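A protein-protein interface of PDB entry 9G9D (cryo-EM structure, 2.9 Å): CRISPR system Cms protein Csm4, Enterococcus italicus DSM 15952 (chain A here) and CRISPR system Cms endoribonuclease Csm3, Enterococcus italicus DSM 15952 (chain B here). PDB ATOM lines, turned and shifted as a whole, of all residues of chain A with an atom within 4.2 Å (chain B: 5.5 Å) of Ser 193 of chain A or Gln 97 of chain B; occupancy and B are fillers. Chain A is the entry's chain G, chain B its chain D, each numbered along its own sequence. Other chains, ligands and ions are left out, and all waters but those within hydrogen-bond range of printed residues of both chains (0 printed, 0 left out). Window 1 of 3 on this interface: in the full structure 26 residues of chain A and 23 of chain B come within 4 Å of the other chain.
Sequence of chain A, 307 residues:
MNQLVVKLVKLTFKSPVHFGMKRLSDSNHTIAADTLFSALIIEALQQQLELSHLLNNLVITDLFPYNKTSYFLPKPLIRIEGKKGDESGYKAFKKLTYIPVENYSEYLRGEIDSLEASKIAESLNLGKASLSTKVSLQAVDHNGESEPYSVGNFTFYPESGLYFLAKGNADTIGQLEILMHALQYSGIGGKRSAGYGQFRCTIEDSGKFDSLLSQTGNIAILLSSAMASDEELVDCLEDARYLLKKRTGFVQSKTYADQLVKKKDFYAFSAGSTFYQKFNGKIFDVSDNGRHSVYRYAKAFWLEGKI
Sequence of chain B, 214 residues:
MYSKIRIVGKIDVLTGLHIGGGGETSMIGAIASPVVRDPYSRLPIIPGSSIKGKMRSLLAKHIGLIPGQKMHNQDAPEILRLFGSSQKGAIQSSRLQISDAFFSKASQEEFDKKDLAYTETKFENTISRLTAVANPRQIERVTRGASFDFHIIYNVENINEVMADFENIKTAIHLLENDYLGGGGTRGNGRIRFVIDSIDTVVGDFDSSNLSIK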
ATOM      1  N   TYR A 185       1.411  -6.445   3.781  1.00  0.00           N
ATOM      2  CA  TYR A 185       1.564  -5.837   2.466  1.00  0.00           C
ATOM      3  C   TYR A 185       2.815  -4.973   2.397  1.00  0.00           C
ATOM      4  O   TYR A 185       3.405  -4.810   1.322  1.00  0.00           O
ATOM      5  CB  TYR A 185       0.313  -5.034   2.128  1.00  0.00           C
ATOM      6  CG  TYR A 185      -0.944  -5.850   2.291  1.00  0.00           C
ATOM      7  CD1 TYR A 185      -1.326  -6.765   1.321  1.00  0.00           C
ATOM      8  CD2 TYR A 185      -1.732  -5.729   3.426  1.00  0.00           C
ATOM      9  CE1 TYR A 185      -2.466  -7.522   1.469  1.00  0.00           C
ATOM     10  CE2 TYR A 185      -2.876  -6.484   3.582  1.00  0.00           C
ATOM     11  CZ  TYR A 185      -3.238  -7.380   2.599  1.00  0.00           C
ATOM     12  OH  TYR A 185      -4.377  -8.137   2.744  1.00  0.00           O
ATOM     13  N   SER A 186       3.236  -4.405   3.533  1.00  0.00           N
ATOM     14  CA  SER A 186       4.510  -3.691   3.562  1.00  0.00           C
ATOM     15  C   SER A 186       5.677  -4.628   3.276  1.00  0.00           C
ATOM     16  O   SER A 186       6.586  -4.285   2.514  1.00  0.00           O
ATOM     17  CB  SER A 186       4.707  -3.002   4.910  1.00  0.00           C
ATOM     18  OG  SER A 186       4.042  -1.754   4.953  1.00  0.00           O
ATOM     19  N   LYS A 191      15.078  -5.539  -0.281  1.00  0.00           N
ATOM     20  CA  LYS A 191      14.479  -5.435  -1.612  1.00  0.00           C
ATOM     21  C   LYS A 191      12.965  -5.619  -1.595  1.00  0.00           C
ATOM     22  O   LYS A 191      12.364  -5.979  -2.608  1.00  0.00           O
ATOM     23  CB  LYS A 191      15.128  -6.411  -2.595  1.00  0.00           C
ATOM     24  CG  LYS A 191      16.432  -5.887  -3.158  1.00  0.00           C
ATOM     25  CD  LYS A 191      16.247  -4.462  -3.663  1.00  0.00           C
ATOM     26  CE  LYS A 191      17.569  -3.802  -4.014  1.00  0.00           C
ATOM     27  NZ  LYS A 191      18.279  -4.517  -5.103  1.00  0.00           N
ATOM     28  N   ARG A 192      12.330  -5.365  -0.456  1.00  0.00           N
ATOM     29  CA  ARG A 192      10.893  -5.166  -0.470  1.00  0.00           C
ATOM     30  C   ARG A 192      10.588  -3.901  -1.262  1.00  0.00           C
ATOM     31  O   ARG A 192      11.444  -3.027  -1.424  1.00  0.00           O
ATOM     32  CB  ARG A 192      10.342  -5.061   0.950  1.00  0.00           C
ATOM     33  CG  ARG A 192      10.792  -3.822   1.693  1.00  0.00           C
ATOM     34  CD  ARG A 192      10.071  -3.688   3.013  1.00  0.00           C
ATOM     35  NE  ARG A 192      10.334  -2.404   3.648  1.00  0.00           N
ATOM     36  CZ  ARG A 192       9.615  -1.309   3.444  1.00  0.00           C
ATOM     37  NH1 ARG A 192       8.590  -1.302   2.611  1.00  0.00           N
ATOM     38  NH2 ARG A 192       9.934  -0.195   4.095  1.00  0.00           N
ATOM     39  N   SER A 193       9.365  -3.816  -1.777  1.00  0.00           N
ATOM     40  CA  SER A 193       8.944  -2.795  -2.734  1.00  0.00           C
ATOM     41  C   SER A 193       9.736  -2.931  -4.026  1.00  0.00           C
ATOM     42  O   SER A 193       9.748  -1.999  -4.843  1.00  0.00           O
ATOM     43  CB  SER A 193       9.078  -1.366  -2.191  1.00  0.00           C
ATOM     44  OG  SER A 193      10.437  -0.999  -2.047  1.00  0.00           O
ATOM     45  N   ALA A 194      10.409  -4.069  -4.231  1.00  0.00           N
ATOM     46  CA  ALA A 194      11.058  -4.405  -5.491  1.00  0.00           C
ATOM     47  C   ALA A 194      10.858  -5.875  -5.843  1.00  0.00           C
ATOM     48  O   ALA A 194      11.662  -6.441  -6.588  1.00  0.00           O
ATOM     49  CB  ALA A 194      12.550  -4.070  -5.447  1.00  0.00           C
ATOM     50  N   GLY A 195       9.817  -6.507  -5.305  1.00  0.00           N
ATOM     51  CA  GLY A 195       9.453  -7.856  -5.687  1.00  0.00           C
ATOM     52  C   GLY A 195       9.639  -8.935  -4.643  1.00  0.00           C
ATOM     53  O   GLY A 195       9.347 -10.101  -4.933  1.00  0.00           O
ATOM     54  N   LYS B   4      -3.177   1.543   1.619  1.00  0.00           N
ATOM     55  CA  LYS B   4      -2.542   0.682   0.635  1.00  0.00           C
ATOM     56  C   LYS B   4      -3.607   0.113  -0.288  1.00  0.00           C
ATOM     57  O   LYS B   4      -4.689  -0.274   0.162  1.00  0.00           O
ATOM     58  CB  LYS B   4      -1.760  -0.445   1.303  1.00  0.00           C
ATOM     59  CG  LYS B   4      -0.561   0.043   2.087  1.00  0.00           C
ATOM     60  CD  LYS B   4       0.102  -1.076   2.856  1.00  0.00           C
ATOM     61  CE  LYS B   4       1.278  -0.543   3.648  1.00  0.00           C
ATOM     62  NZ  LYS B   4       1.822  -1.573   4.564  1.00  0.00           N
ATOM     63  N   LYS B  52       8.622  -3.461 -12.534  1.00  0.00           N
ATOM     64  CA  LYS B  52       8.829  -2.124 -11.985  1.00  0.00           C
ATOM     65  C   LYS B  52       9.788  -1.318 -12.851  1.00  0.00           C
ATOM     66  O   LYS B  52       9.540  -0.146 -13.151  1.00  0.00           O
ATOM     67  CB  LYS B  52       9.352  -2.222 -10.551  1.00  0.00           C
ATOM     68  CG  LYS B  52       9.555  -0.884  -9.865  1.00  0.00           C
ATOM     69  CD  LYS B  52      10.166  -1.061  -8.486  1.00  0.00           C
ATOM     70  CE  LYS B  52      10.259   0.260  -7.743  1.00  0.00           C
ATOM     71  NZ  LYS B  52      11.094   0.152  -6.516  1.00  0.00           N
ATOM     72  N   SER B  94       9.346   4.039  -2.312  1.00  0.00           N
ATOM     73  CA  SER B  94       8.671   3.602  -3.526  1.00  0.00           C
ATOM     74  C   SER B  94       7.204   3.324  -3.235  1.00  0.00           C
ATOM     75  O   SER B  94       6.873   2.593  -2.297  1.00  0.00           O
ATOM     76  CB  SER B  94       9.343   2.352  -4.090  1.00  0.00           C
ATOM     77  OG  SER B  94       8.725   1.945  -5.297  1.00  0.00           O
ATOM     78  N   ARG B  95       6.322   3.916  -4.041  1.00  0.00           N
ATOM     79  CA  ARG B  95       4.894   3.703  -3.844  1.00  0.00           C
ATOM     80  C   ARG B  95       4.441   2.392  -4.470  1.00  0.00           C
ATOM     81  O   ARG B  95       3.550   1.720  -3.940  1.00  0.00           O
ATOM     82  CB  ARG B  95       4.103   4.879  -4.413  1.00  0.00           C
ATOM     83  CG  ARG B  95       4.467   6.212  -3.789  1.00  0.00           C
ATOM     84  CD  ARG B  95       3.383   7.247  -4.012  1.00  0.00           C
ATOM     85  NE  ARG B  95       3.754   8.545  -3.464  1.00  0.00           N
ATOM     86  CZ  ARG B  95       2.943   9.594  -3.405  1.00  0.00           C
ATOM     87  NH1 ARG B  95       1.694   9.524  -3.832  1.00  0.00           N
ATOM     88  NH2 ARG B  95       3.397  10.738  -2.903  1.00  0.00           N
ATOM     89  N   LEU B  96       5.039   2.011  -5.594  1.00  0.00           N
ATOM     90  CA  LEU B  96       4.698   0.775  -6.284  1.00  0.00           C
ATOM     91  C   LEU B  96       5.591  -0.353  -5.792  1.00  0.00           C
ATOM     92  O   LEU B  96       6.798  -0.356  -6.053  1.00  0.00           O
ATOM     93  CB  LEU B  96       4.835   0.926  -7.799  1.00  0.00           C
ATOM     94  CG  LEU B  96       3.687   1.630  -8.517  1.00  0.00           C
ATOM     95  CD1 LEU B  96       3.768   1.364 -10.008  1.00  0.00           C
ATOM     96  CD2 LEU B  96       2.352   1.176  -7.960  1.00  0.00           C
ATOM     97  N   GLN B  97       4.996  -1.246  -5.000  1.00  0.00           N
ATOM     98  CA  GLN B  97       5.722  -2.454  -4.549  1.00  0.00           C
ATOM     99  C   GLN B  97       5.147  -3.593  -5.390  1.00  0.00           C
ATOM    100  O   GLN B  97       4.006  -4.011  -5.104  1.00  0.00           O
ATOM    101  CB  GLN B  97       5.456  -2.741  -3.074  1.00  0.00           C
ATOM    102  CG  GLN B  97       5.441  -1.506  -2.183  1.00  0.00           C
ATOM    103  CD  GLN B  97       5.163  -1.837  -0.733  1.00  0.00           C
ATOM    104  OE1 GLN B  97       5.122  -0.957   0.133  1.00  0.00           O
ATOM    105  NE2 GLN B  97       4.967  -3.118  -0.455  1.00  0.00           N
ATOM    106  N   ILE B  98       5.886  -4.068  -6.391  1.00  0.00           N
ATOM    107  CA  ILE B  98       5.276  -5.081  -7.297  1.00  0.00           C
ATOM    108  C   ILE B  98       5.873  -6.454  -6.972  1.00  0.00           C
ATOM    109  O   ILE B  98       7.095  -6.604  -7.120  1.00  0.00           O
ATOM    110  CB  ILE B  98       5.538  -4.692  -8.762  1.00  0.00           C
ATOM    111  CG1 ILE B  98       5.148  -3.240  -9.037  1.00  0.00           C
ATOM    112  CG2 ILE B  98       4.846  -5.660  -9.722  1.00  0.00           C
ATOM    113  CD1 ILE B  98       5.424  -2.785 -10.459  1.00  0.00           C
ATOM    114  N   SER B  99       5.024  -7.419  -6.616  1.00  0.00           N
ATOM    115  CA  SER B  99       5.479  -8.796  -6.295  1.00  0.00           C
ATOM    116  C   SER B  99       5.912  -9.506  -7.583  1.00  0.00           C
ATOM    117  O   SER B  99       5.392  -9.139  -8.658  1.00  0.00           O
ATOM    118  CB  SER B  99       4.397  -9.558  -5.583  1.00  0.00           C
ATOM    119  OG  SER B  99       3.908  -8.820  -4.472  1.00  0.00           O
ATOM    120  N   HIS B 151       0.654  -9.081  -8.474  1.00  0.00           N
ATOM    121  CA  HIS B 151       0.135  -8.333  -7.301  1.00  0.00           C
ATOM    122  C   HIS B 151       0.955  -7.046  -7.199  1.00  0.00           C
ATOM    123  O   HIS B 151       2.202  -7.117  -7.190  1.00  0.00           O
ATOM    124  CB  HIS B 151       0.192  -9.230  -6.059  1.00  0.00           C
ATOM    125  CG  HIS B 151       0.089  -8.533  -4.748  1.00  0.00           C
ATOM    126  ND1 HIS B 151       0.737  -9.013  -3.632  1.00  0.00           N
ATOM    127  CD2 HIS B 151      -0.555  -7.430  -4.356  1.00  0.00           C
ATOM    128  CE1 HIS B 151       0.484  -8.219  -2.604  1.00  0.00           C
ATOM    129  NE2 HIS B 151      -0.299  -7.252  -3.023  1.00  0.00           N
ATOM    130  N   ILE B 152       0.277  -5.900  -7.154  1.00  0.00           N
ATOM    131  CA  ILE B 152       1.001  -4.606  -6.992  1.00  0.00           C
ATOM    132  C   ILE B 152       0.430  -3.898  -5.758  1.00  0.00           C
ATOM    133  O   ILE B 152      -0.808  -3.853  -5.632  1.00  0.00           O
ATOM    134  CB  ILE B 152       0.872  -3.735  -8.255  1.00  0.00           C
ATOM    135  CG1 ILE B 152       1.352  -4.470  -9.503  1.00  0.00           C
ATOM    136  CG2 ILE B 152       1.597  -2.403  -8.075  1.00  0.00           C
ATOM    137  CD1 ILE B 152       1.375  -3.609 -10.752  1.00  0.00           C
ATOM    138  N   ILE B 153       1.296  -3.399  -4.875  1.00  0.00           N
ATOM    139  CA  ILE B 153       0.792  -2.611  -3.712  1.00  0.00           C
ATOM    140  C   ILE B 153       1.104  -1.131  -3.960  1.00  0.00           C
ATOM    141  O   ILE B 153       2.296  -0.804  -4.114  1.00  0.00           O
ATOM    142  CB  ILE B 153       1.381  -3.102  -2.376  1.00  0.00           C
ATOM    143  CG1 ILE B 153       0.701  -4.375  -1.907  1.00  0.00           C
ATOM    144  CG2 ILE B 153       1.296  -2.015  -1.305  1.00  0.00           C
ATOM    145  CD1 ILE B 153      -0.748  -4.176  -1.507  1.00  0.00           C
ATOM    146  N   TYR B 154       0.072  -0.296  -4.084  1.00  0.00           N
ATOM    147  CA  TYR B 154       0.296   1.139  -4.178  1.00  0.00           C
ATOM    148  C   TYR B 154       0.143   1.740  -2.789  1.00  0.00           C
ATOM    149  O   TYR B 154      -0.876   1.525  -2.126  1.00  0.00           O
ATOM    150  CB  TYR B 154      -0.672   1.801  -5.158  1.00  0.00           C
ATOM    151  CG  TYR B 154      -0.510   3.301  -5.205  1.00  0.00           C
ATOM    152  CD1 TYR B 154       0.473   3.886  -5.990  1.00  0.00           C
ATOM    153  CD2 TYR B 154      -1.324   4.131  -4.449  1.00  0.00           C
ATOM    154  CE1 TYR B 154       0.631   5.253  -6.027  1.00  0.00           C
ATOM    155  CE2 TYR B 154      -1.172   5.499  -4.479  1.00  0.00           C
ATOM    156  CZ  TYR B 154      -0.193   6.056  -5.270  1.00  0.00           C
ATOM    157  OH  TYR B 154      -0.043   7.422  -5.301  1.00  0.00           O
ATOM    158  N   ASN B 155       1.145   2.496  -2.358  1.00  0.00           N
ATOM    159  CA  ASN B 155       1.129   3.122  -1.044  1.00  0.00           C
ATOM    160  C   ASN B 155       0.675   4.568  -1.188  1.00  0.00           C
ATOM    161  O   ASN B 155       1.292   5.347  -1.921  1.00  0.00           O
ATOM    162  CB  ASN B 155       2.511   3.051  -0.401  1.00  0.00           C
ATOM    163  CG  ASN B 155       3.010   1.632  -0.254  1.00  0.00           C
ATOM    164  OD1 ASN B 155       2.732   0.966   0.742  1.00  0.00           O
ATOM    165  ND2 ASN B 155       3.753   1.160  -1.247  1.00  0.00           N
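The side-chain amino group (NZ) of Lys 52 of chain B sits at hydrogen-bond distance from the backbone carbonyl oxygen (O) of Ser 193 of chain A, 3.0 Å away. O of Tyr 185 of chain A sits at hydrogen-bond distance from NE2 of Gln 97 of chain B (2.9 Å). O of Ile 98 of chain B lies close to N of Gly 195 of chain A. The side-chain hydroxyl (OG) of Ser 186 of chain A sits close to the side-chain amino group (NZ) of Lys 4 of chain B.
NZ of Lys 52 of chain B is in hydrogen-bond range of OG of Ser 94 of chain B (3.2 Å). The side-chain hydroxyl (OG) of Ser 94 of chain B is in hydrogen-bond range of the backbone carbonyl oxygen (O) of Leu 96 of chain B. The backbone NH of Ile 153 of chain B sits at hydrogen-bond distance from the backbone carbonyl oxygen of Gln 97 of chain B, at 2.8 Å. The side-chain amide oxygen of Gln 97 of chain B sits at hydrogen-bond distance from the side-chain amide nitrogen of Asn 155 of chain B, 2.9 Å away.
Among the printed residues, pairs that only touch across the chains: Ser 193 of chain A with Gln 97 of chain B (3.5 Å), Ser 186 of chain A with Gln 97 of chain B (3.6 Å), Ser 193 of chain A with Leu 96 of chain B (3.6 Å) and Tyr 185 of chain A with Ile 153 of chain B (3.9 Å).
Gln 97 of chain B touches just these residues of chain A: Tyr 185 (2.9 Å), Ser 186 (3.6 Å) and Ser 193 (3.5 Å). Of the printed residues of chain A, Lys 4 of chain B touches Ser 186 (2.3 Å). Printed residues of chain A within 4 Å of Leu 96 of chain B: Ser 193. Of the printed residues of chain B, Tyr 185 of chain A touches Gln 97 and Ile 153. Arg 95 of chain B touches none of the printed residues of chain A. Asn 155 of chain B touches none of the printed residues of chain A. The nearest printed residue of chain A that does not touch Gln 97 of chain B is Arg 192 of chain A (4.3 Å).
Of the 13 printed residues of chain B, 6 touch a printed residue of chain A. Printed residues of chain B that touch a printed residue of chain A: Lys 4, Lys 52, Leu 96, Gln 97, Ile 98 and Ile 153. Hydrophobic or aromatic side chains of chain A that line the printed part of chain B: Tyr 185. Along chain A the printed residues that touch a printed residue of chain B span positions 185 to 195. Among the printed residues, 8 pairs touch across the chains. Among the printed residues, no Asp or Glu carboxylate lies within 4 Å of a Lys or Arg side-chain nitrogen of the other chain.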
